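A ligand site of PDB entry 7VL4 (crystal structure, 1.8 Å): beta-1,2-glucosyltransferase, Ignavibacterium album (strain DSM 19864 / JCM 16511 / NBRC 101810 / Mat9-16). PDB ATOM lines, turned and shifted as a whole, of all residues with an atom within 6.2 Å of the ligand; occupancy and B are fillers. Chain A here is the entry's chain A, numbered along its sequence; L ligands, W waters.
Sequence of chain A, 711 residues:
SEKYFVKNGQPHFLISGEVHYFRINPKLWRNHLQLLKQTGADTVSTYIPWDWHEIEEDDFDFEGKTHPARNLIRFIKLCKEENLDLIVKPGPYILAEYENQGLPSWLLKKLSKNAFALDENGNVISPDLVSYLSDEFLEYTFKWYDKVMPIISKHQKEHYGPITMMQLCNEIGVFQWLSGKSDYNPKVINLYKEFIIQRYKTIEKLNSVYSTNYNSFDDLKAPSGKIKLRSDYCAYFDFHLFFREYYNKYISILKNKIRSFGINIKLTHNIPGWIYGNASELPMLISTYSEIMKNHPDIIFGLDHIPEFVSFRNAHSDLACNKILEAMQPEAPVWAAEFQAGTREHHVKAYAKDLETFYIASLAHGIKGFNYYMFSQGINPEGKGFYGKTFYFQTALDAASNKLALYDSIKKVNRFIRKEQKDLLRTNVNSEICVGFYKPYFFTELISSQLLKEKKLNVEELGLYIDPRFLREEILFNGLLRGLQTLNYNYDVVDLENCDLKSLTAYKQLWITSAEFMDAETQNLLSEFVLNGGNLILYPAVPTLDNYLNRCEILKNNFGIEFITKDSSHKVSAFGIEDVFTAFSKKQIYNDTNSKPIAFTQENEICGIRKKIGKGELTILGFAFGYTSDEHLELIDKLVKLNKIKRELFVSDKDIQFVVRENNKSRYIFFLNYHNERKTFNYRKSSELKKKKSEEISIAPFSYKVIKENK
Water W2 lies within hydrogen-bond range of the side-chain carboxylate (OE1) of Glu 97 (2.6 Å), an oxygen (O1) of the ligand (2.7 Å) and the guanidinium group (NH2) of Arg 344 (3.0 Å).
Water W3 lies within hydrogen-bond range of the backbone carbonyl oxygen (O) of Asp 304 (2.7 Å), an oxygen (O3) of the ligand (2.8 Å), the backbone NH (N) of Trp 274 (2.9 Å) and the backbone NH (N) of Gly 273 (3.2 Å).
Water W1 lies within hydrogen-bond range of OE1 of Glu 338 (2.9 Å) and O2 of the ligand (3.1 Å).
Leu 95 touches the ligand (CD1 to O2, 3.4 Å).
CZ3 of Trp 177 touches O4 of the ligand, at 3.7 Å.
CD1 of Leu 178 touches C7 of the ligand, at 3.7 Å.
Pro 272 touches the ligand.
Ile 275 touches the ligand.
Asp 304 touches the ligand.
CD1 of Ile 306 touches O3 of the ligand, 3.8 Å away.
Hydrophobic or aromatic side chains within 4 Å of the ligand: Leu 95, Trp 177, Leu 178, Pro 272, Ile 275 and Ile 306.
Within 4 Å of the ligand: Leu 95, Glu 171, Trp 177, Leu 178, Pro 272, Gly 273, Trp 274, Ile 275, Asp 304, Ile 306 and Arg 344.
The nearest printed residue that does not touch the ligand is Val 174 (4.3 Å).
The side-chain amide nitrogen (ND2) of Asn 170 is in hydrogen-bond range of the side-chain carboxylate (OE2) of Glu 171 (2.8 Å).
The side-chain carboxylate (OD1) of Asp 304 lies within hydrogen-bond range of the backbone NH (N) of Glu 338.
The backbone carbonyl oxygen of Ile 271 lies within hydrogen-bond range of the backbone NH of Asp 304 (3.0 Å).
O of Gln 101 sits at hydrogen-bond distance from N of Leu 95 (3.1 Å).
An oxygen (O6) of the ligand lies within hydrogen-bond range of the guanidinium group (NH1) of Arg 344, at 2.8 Å.
N of Trp 274 lies within hydrogen-bond range of O4 of the ligand (3.3 Å).
The side-chain carboxylate of Glu 171 lies within hydrogen-bond range of an oxygen (O2) of the ligand (2.7 Å).
O of Trp 274 is in hydrogen-bond range of O4 of the ligand (2.7 Å).
The backbone NH (N) of Gly 273 sits at hydrogen-bond distance from an oxygen (O4) of the ligand (3.0 Å).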
ATOM      1  N   LEU A  95      -5.248   5.398  11.173  1.00  0.00           N
ATOM      2  CA  LEU A  95      -4.536   4.867  12.361  1.00  0.00           C
ATOM      3  C   LEU A  95      -4.636   3.336  12.275  1.00  0.00           C
ATOM      4  O   LEU A  95      -3.884   2.780  11.480  1.00  0.00           O
ATOM      5  CB  LEU A  95      -5.157   5.471  13.634  1.00  0.00           C
ATOM      6  CG  LEU A  95      -4.319   5.431  14.907  1.00  0.00           C
ATOM      7  CD1 LEU A  95      -4.926   6.353  15.978  1.00  0.00           C
ATOM      8  CD2 LEU A  95      -4.210   4.023  15.473  1.00  0.00           C
ATOM      9  N   GLU A  97      -3.680   0.695  13.555  1.00  0.00           N
ATOM     10  CA  GLU A  97      -2.411  -0.093  13.657  1.00  0.00           C
ATOM     11  C   GLU A  97      -1.947  -0.484  12.250  1.00  0.00           C
ATOM     12  O   GLU A  97      -1.484  -1.628  12.020  1.00  0.00           O
ATOM     13  CB  GLU A  97      -2.589  -1.311  14.566  1.00  0.00           C
ATOM     14  CG  GLU A  97      -2.603  -0.979  16.045  1.00  0.00           C
ATOM     15  CD  GLU A  97      -3.845  -0.255  16.564  1.00  0.00           C
ATOM     16  OE1 GLU A  97      -3.690   0.598  17.455  1.00  0.00           O
ATOM     17  OE2 GLU A  97      -4.953  -0.556  16.081  1.00  0.00           O
ATOM     18  N   GLN A 101      -0.112   4.906   9.504  1.00  0.00           N
ATOM     19  CA  GLN A 101      -1.492   5.319   9.908  1.00  0.00           C
ATOM     20  C   GLN A 101      -2.480   5.264   8.701  1.00  0.00           C
ATOM     21  O   GLN A 101      -3.474   5.997   8.733  1.00  0.00           O
ATOM     22  CB  GLN A 101      -1.436   6.708  10.532  1.00  0.00           C
ATOM     23  CG  GLN A 101      -0.259   6.927  11.495  1.00  0.00           C
ATOM     24  CD  GLN A 101      -0.274   5.960  12.652  1.00  0.00           C
ATOM     25  OE1 GLN A 101      -1.293   5.374  12.988  1.00  0.00           O
ATOM     26  NE2 GLN A 101       0.858   5.805  13.318  1.00  0.00           N
ATOM     27  N   ASN A 170      -9.783  10.516  10.983  1.00  0.00           N
ATOM     28  CA  ASN A 170      -9.734   9.647  12.194  1.00  0.00           C
ATOM     29  C   ASN A 170      -9.093  10.446  13.331  1.00  0.00           C
ATOM     30  O   ASN A 170      -7.935  10.886  13.114  1.00  0.00           O
ATOM     31  CB  ASN A 170      -8.970   8.352  11.946  1.00  0.00           C
ATOM     32  CG  ASN A 170      -9.155   7.358  13.071  1.00  0.00           C
ATOM     33  OD1 ASN A 170     -10.172   6.667  13.135  1.00  0.00           O
ATOM     34  ND2 ASN A 170      -8.186   7.302  13.984  1.00  0.00           N
ATOM     35  N   GLU A 171      -9.833  10.673  14.430  1.00  0.00           N
ATOM     36  CA  GLU A 171      -9.317  11.282  15.689  1.00  0.00           C
ATOM     37  C   GLU A 171      -8.401  12.468  15.378  1.00  0.00           C
ATOM     38  O   GLU A 171      -7.183  12.446  15.685  1.00  0.00           O
ATOM     39  CB  GLU A 171      -8.616  10.192  16.510  1.00  0.00           C
ATOM     40  CG  GLU A 171      -9.450   8.932  16.694  1.00  0.00           C
ATOM     41  CD  GLU A 171      -8.606   7.718  17.096  1.00  0.00           C
ATOM     42  OE1 GLU A 171      -7.611   7.983  17.762  1.00  0.00           O
ATOM     43  OE2 GLU A 171      -8.883   6.516  16.574  1.00  0.00           O
ATOM     44  N   VAL A 174      -5.032  13.338  17.184  1.00  0.00           N
ATOM     45  CA  VAL A 174      -4.522  12.229  18.036  1.00  0.00           C
ATOM     46  C   VAL A 174      -3.011  12.060  17.829  1.00  0.00           C
ATOM     47  O   VAL A 174      -2.280  11.860  18.826  1.00  0.00           O
ATOM     48  CB  VAL A 174      -5.289  10.906  17.812  1.00  0.00           C
ATOM     49  CG1 VAL A 174      -4.948  10.220  16.503  1.00  0.00           C
ATOM     50  CG2 VAL A 174      -5.050   9.957  18.981  1.00  0.00           C
ATOM     51  N   PHE A 175      -2.545  12.114  16.588  1.00  0.00           N
ATOM     52  CA  PHE A 175      -1.126  11.871  16.227  1.00  0.00           C
ATOM     53  C   PHE A 175      -0.297  12.989  16.822  1.00  0.00           C
ATOM     54  O   PHE A 175       0.735  12.712  17.395  1.00  0.00           O
ATOM     55  CB  PHE A 175      -0.907  11.707  14.713  1.00  0.00           C
ATOM     56  CG  PHE A 175      -1.783  10.665  14.075  1.00  0.00           C
ATOM     57  CD1 PHE A 175      -1.626   9.326  14.397  1.00  0.00           C
ATOM     58  CD2 PHE A 175      -2.797  11.031  13.220  1.00  0.00           C
ATOM     59  CE1 PHE A 175      -2.485   8.367  13.867  1.00  0.00           C
ATOM     60  CE2 PHE A 175      -3.650  10.075  12.674  1.00  0.00           C
ATOM     61  CZ  PHE A 175      -3.488   8.744  12.993  1.00  0.00           C
ATOM     62  N   TRP A 177      -1.022  14.819  19.479  1.00  0.00           N
ATOM     63  CA  TRP A 177      -1.116  14.580  20.942  1.00  0.00           C
ATOM     64  C   TRP A 177      -0.106  13.498  21.356  1.00  0.00           C
ATOM     65  O   TRP A 177       0.686  13.756  22.235  1.00  0.00           O
ATOM     66  CB  TRP A 177      -2.577  14.227  21.281  1.00  0.00           C
ATOM     67  CG  TRP A 177      -2.834  13.784  22.696  1.00  0.00           C
ATOM     68  CD1 TRP A 177      -2.626  14.489  23.850  1.00  0.00           C
ATOM     69  CD2 TRP A 177      -3.456  12.545  23.066  1.00  0.00           C
ATOM     70  NE1 TRP A 177      -3.019  13.728  24.928  1.00  0.00           N
ATOM     71  CE2 TRP A 177      -3.574  12.555  24.467  1.00  0.00           C
ATOM     72  CE3 TRP A 177      -3.940  11.447  22.346  1.00  0.00           C
ATOM     73  CZ2 TRP A 177      -4.102  11.478  25.171  1.00  0.00           C
ATOM     74  CZ3 TRP A 177      -4.476  10.394  23.034  1.00  0.00           C
ATOM     75  CH2 TRP A 177      -4.535  10.404  24.431  1.00  0.00           C
ATOM     76  N   LEU A 178      -0.151  12.333  20.740  1.00  0.00           N
ATOM     77  CA  LEU A 178       0.706  11.171  21.103  1.00  0.00           C
ATOM     78  C   LEU A 178       2.202  11.459  20.817  1.00  0.00           C
ATOM     79  O   LEU A 178       3.042  10.906  21.536  1.00  0.00           O
ATOM     80  CB  LEU A 178       0.219   9.952  20.333  1.00  0.00           C
ATOM     81  CG  LEU A 178      -1.126   9.384  20.797  1.00  0.00           C
ATOM     82  CD1 LEU A 178      -1.510   8.214  19.913  1.00  0.00           C
ATOM     83  CD2 LEU A 178      -1.066   8.908  22.222  1.00  0.00           C
ATOM     84  N   ILE A 271     -13.696  10.389  18.811  1.00  0.00           N
ATOM     85  CA  ILE A 271     -13.002  11.140  19.892  1.00  0.00           C
ATOM     86  C   ILE A 271     -12.023  10.208  20.590  1.00  0.00           C
ATOM     87  O   ILE A 271     -12.424   9.255  21.284  1.00  0.00           O
ATOM     88  CB  ILE A 271     -13.997  11.726  20.907  1.00  0.00           C
ATOM     89  CG1 ILE A 271     -15.054  12.621  20.246  1.00  0.00           C
ATOM     90  CG2 ILE A 271     -13.205  12.494  21.960  1.00  0.00           C
ATOM     91  CD1 ILE A 271     -16.303  12.801  21.079  1.00  0.00           C
ATOM     92  N   PRO A 272     -10.707  10.534  20.519  1.00  0.00           N
ATOM     93  CA  PRO A 272      -9.697   9.790  21.268  1.00  0.00           C
ATOM     94  C   PRO A 272      -9.546  10.337  22.709  1.00  0.00           C
ATOM     95  O   PRO A 272     -10.089  11.378  23.043  1.00  0.00           O
ATOM     96  CB  PRO A 272      -8.455  10.118  20.429  1.00  0.00           C
ATOM     97  CG  PRO A 272      -8.652  11.581  20.078  1.00  0.00           C
ATOM     98  CD  PRO A 272     -10.141  11.692  19.798  1.00  0.00           C
ATOM     99  N   GLY A 273      -8.806   9.644  23.565  1.00  0.00           N
ATOM    100  CA  GLY A 273      -8.374  10.215  24.853  1.00  0.00           C
ATOM    101  C   GLY A 273      -8.130   9.145  25.906  1.00  0.00           C
ATOM    102  O   GLY A 273      -7.537   9.478  26.918  1.00  0.00           O
ATOM    103  N   TRP A 274      -8.590   7.922  25.715  1.00  0.00           N
ATOM    104  CA  TRP A 274      -8.293   6.862  26.707  1.00  0.00           C
ATOM    105  C   TRP A 274      -6.829   6.464  26.528  1.00  0.00           C
ATOM    106  O   TRP A 274      -6.331   6.399  25.397  1.00  0.00           O
ATOM    107  CB  TRP A 274      -9.185   5.643  26.582  1.00  0.00           C
ATOM    108  CG  TRP A 274     -10.607   5.776  27.017  1.00  0.00           C
ATOM    109  CD1 TRP A 274     -11.598   6.376  26.309  1.00  0.00           C
ATOM    110  CD2 TRP A 274     -11.241   5.184  28.172  1.00  0.00           C
ATOM    111  NE1 TRP A 274     -12.796   6.248  26.935  1.00  0.00           N
ATOM    112  CE2 TRP A 274     -12.621   5.482  28.061  1.00  0.00           C
ATOM    113  CE3 TRP A 274     -10.789   4.447  29.269  1.00  0.00           C
ATOM    114  CZ2 TRP A 274     -13.543   5.097  29.038  1.00  0.00           C
ATOM    115  CZ3 TRP A 274     -11.692   4.054  30.220  1.00  0.00           C
ATOM    116  CH2 TRP A 274     -13.059   4.342  30.099  1.00  0.00           C
ATOM    117  N   ILE A 275      -6.129   6.294  27.648  1.00  0.00           N
ATOM    118  CA  ILE A 275      -4.768   5.739  27.582  1.00  0.00           C
ATOM    119  C   ILE A 275      -4.521   4.999  28.906  1.00  0.00           C
ATOM    120  O   ILE A 275      -4.923   5.508  29.978  1.00  0.00           O
ATOM    121  CB  ILE A 275      -3.766   6.835  27.225  1.00  0.00           C
ATOM    122  CG1 ILE A 275      -2.397   6.219  26.926  1.00  0.00           C
ATOM    123  CG2 ILE A 275      -3.734   7.923  28.291  1.00  0.00           C
ATOM    124  CD1 ILE A 275      -1.349   7.197  26.424  1.00  0.00           C
ATOM    125  N   TYR A 276      -3.966   3.807  28.825  1.00  0.00           N
ATOM    126  CA  TYR A 276      -3.691   2.961  30.007  1.00  0.00           C
ATOM    127  C   TYR A 276      -4.990   2.693  30.769  1.00  0.00           C
ATOM    128  O   TYR A 276      -4.916   2.382  31.961  1.00  0.00           O
ATOM    129  CB  TYR A 276      -2.582   3.577  30.870  1.00  0.00           C
ATOM    130  CG  TYR A 276      -1.381   4.068  30.093  1.00  0.00           C
ATOM    131  CD1 TYR A 276      -0.736   3.233  29.190  1.00  0.00           C
ATOM    132  CD2 TYR A 276      -0.851   5.335  30.290  1.00  0.00           C
ATOM    133  CE1 TYR A 276       0.348   3.661  28.449  1.00  0.00           C
ATOM    134  CE2 TYR A 276       0.248   5.783  29.565  1.00  0.00           C
ATOM    135  CZ  TYR A 276       0.865   4.938  28.656  1.00  0.00           C
ATOM    136  OH  TYR A 276       1.951   5.343  27.923  1.00  0.00           O
ATOM    137  N   ASP A 304     -14.326   6.988  21.417  1.00  0.00           N
ATOM    138  CA  ASP A 304     -13.472   5.785  21.301  1.00  0.00           C
ATOM    139  C   ASP A 304     -13.200   5.284  22.711  1.00  0.00           C
ATOM    140  O   ASP A 304     -12.322   5.854  23.349  1.00  0.00           O
ATOM    141  CB  ASP A 304     -12.227   6.098  20.459  1.00  0.00           C
ATOM    142  CG  ASP A 304     -12.633   6.538  19.060  1.00  0.00           C
ATOM    143  OD1 ASP A 304     -13.824   6.277  18.663  1.00  0.00           O
ATOM    144  OD2 ASP A 304     -11.768   7.114  18.329  1.00  0.00           O
ATOM    145  N   ILE A 306     -11.718   2.841  25.350  1.00  0.00           N
ATOM    146  CA  ILE A 306     -10.669   1.792  25.546  1.00  0.00           C
ATOM    147  C   ILE A 306     -10.374   1.604  27.040  1.00  0.00           C
ATOM    148  O   ILE A 306      -9.318   2.007  27.560  1.00  0.00           O
ATOM    149  CB  ILE A 306      -9.390   2.090  24.764  1.00  0.00           C
ATOM    150  CG1 ILE A 306      -9.676   2.665  23.373  1.00  0.00           C
ATOM    151  CG2 ILE A 306      -8.523   0.848  24.707  1.00  0.00           C
ATOM    152  CD1 ILE A 306      -8.422   2.962  22.620  1.00  0.00           C
ATOM    153  N   GLU A 308      -9.726  -1.219  28.876  1.00  0.00           N
ATOM    154  CA  GLU A 308      -8.676  -2.277  29.045  1.00  0.00           C
ATOM    155  C   GLU A 308      -9.017  -3.228  30.198  1.00  0.00           C
ATOM    156  O   GLU A 308      -8.688  -4.402  30.081  1.00  0.00           O
ATOM    157  CB  GLU A 308      -7.280  -1.687  29.257  1.00  0.00           C
ATOM    158  CG  GLU A 308      -6.834  -0.762  28.151  1.00  0.00           C
ATOM    159  CD  GLU A 308      -5.442  -0.225  28.298  1.00  0.00           C
ATOM    160  OE1 GLU A 308      -4.784  -0.473  29.351  1.00  0.00           O
ATOM    161  OE2 GLU A 308      -5.014   0.478  27.383  1.00  0.00           O
ATOM    162  N   GLU A 338     -15.954   3.675  18.497  1.00  0.00           N
ATOM    163  CA  GLU A 338     -15.120   2.487  18.762  1.00  0.00           C
ATOM    164  C   GLU A 338     -15.358   2.076  20.205  1.00  0.00           C
ATOM    165  O   GLU A 338     -15.149   2.912  21.106  1.00  0.00           O
ATOM    166  CB  GLU A 338     -13.630   2.766  18.516  1.00  0.00           C
ATOM    167  CG  GLU A 338     -13.327   3.265  17.101  1.00  0.00           C
ATOM    168  CD  GLU A 338     -11.887   3.713  16.960  1.00  0.00           C
ATOM    169  OE1 GLU A 338     -11.026   3.130  17.660  1.00  0.00           O
ATOM    170  OE2 GLU A 338     -11.614   4.603  16.114  1.00  0.00           O
ATOM    171  N   ARG A 344      -6.016  -4.192  21.238  1.00  0.00           N
ATOM    172  CA  ARG A 344      -5.093  -3.778  20.154  1.00  0.00           C
ATOM    173  C   ARG A 344      -3.648  -4.257  20.442  1.00  0.00           C
ATOM    174  O   ARG A 344      -2.789  -4.180  19.518  1.00  0.00           O
ATOM    175  CB  ARG A 344      -5.178  -2.255  20.075  1.00  0.00           C
ATOM    176  CG  ARG A 344      -4.628  -1.575  21.319  1.00  0.00           C
ATOM    177  CD  ARG A 344      -4.857  -0.070  21.250  1.00  0.00           C
ATOM    178  NE  ARG A 344      -4.553   0.568  22.537  1.00  0.00           N
ATOM    179  CZ  ARG A 344      -4.480   1.885  22.701  1.00  0.00           C
ATOM    180  NH1 ARG A 344      -4.156   2.417  23.875  1.00  0.00           N
ATOM    181  NH2 ARG A 344      -4.673   2.680  21.677  1.00  0.00           N
ATOM    182  N   TYR A 387       2.786  -2.837  13.982  1.00  0.00           N
ATOM    183  CA  TYR A 387       3.452  -3.383  15.188  1.00  0.00           C
ATOM    184  C   TYR A 387       3.658  -4.910  15.135  1.00  0.00           C
ATOM    185  O   TYR A 387       4.171  -5.420  16.146  1.00  0.00           O
ATOM    186  CB  TYR A 387       2.620  -3.094  16.432  1.00  0.00           C
ATOM    187  CG  TYR A 387       2.555  -1.636  16.830  1.00  0.00           C
ATOM    188  CD1 TYR A 387       3.685  -0.967  17.259  1.00  0.00           C
ATOM    189  CD2 TYR A 387       1.352  -0.942  16.794  1.00  0.00           C
ATOM    190  CE1 TYR A 387       3.652   0.364  17.620  1.00  0.00           C
ATOM    191  CE2 TYR A 387       1.289   0.394  17.151  1.00  0.00           C
ATOM    192  CZ  TYR A 387       2.445   1.046  17.573  1.00  0.00           C
ATOM    193  OH  TYR A 387       2.413   2.368  17.907  1.00  0.00           O
HETATM  194  C1  LIG L   1      -4.864   5.683  19.842  1.00  0.00           C
HETATM  195  C2  LIG L   1      -6.370   5.514  19.893  1.00  0.00           C
HETATM  196  C3  LIG L   1      -7.011   6.589  20.799  1.00  0.00           C
HETATM  197  C4  LIG L   1      -6.270   6.518  22.135  1.00  0.00           C
HETATM  198  C5  LIG L   1      -4.747   6.672  21.985  1.00  0.00           C
HETATM  199  C6  LIG L   1      -4.007   6.497  23.296  1.00  0.00           C
HETATM  200  C7  LIG L   1      -2.871   4.934  18.815  1.00  0.00           C
HETATM  201  O1  LIG L   1      -4.235   4.671  19.086  1.00  0.00           O
HETATM  202  O2  LIG L   1      -6.974   5.541  18.604  1.00  0.00           O
HETATM  203  O3  LIG L   1      -8.438   6.357  20.959  1.00  0.00           O
HETATM  204  O4  LIG L   1      -6.758   7.537  23.002  1.00  0.00           O
HETATM  205  O5  LIG L   1      -4.226   5.670  21.122  1.00  0.00           O
HETATM  206  O6  LIG L   1      -4.381   5.246  23.933  1.00  0.00           O
HETATM  207  O   HOH W   1      -8.307   2.738  18.498  1.00  0.00           O
HETATM  208  O   HOH W   2      -5.260   2.163  18.769  1.00  0.00           O
HETATM  209  O   HOH W   3      -9.680   6.560  23.450  1.00  0.00           O
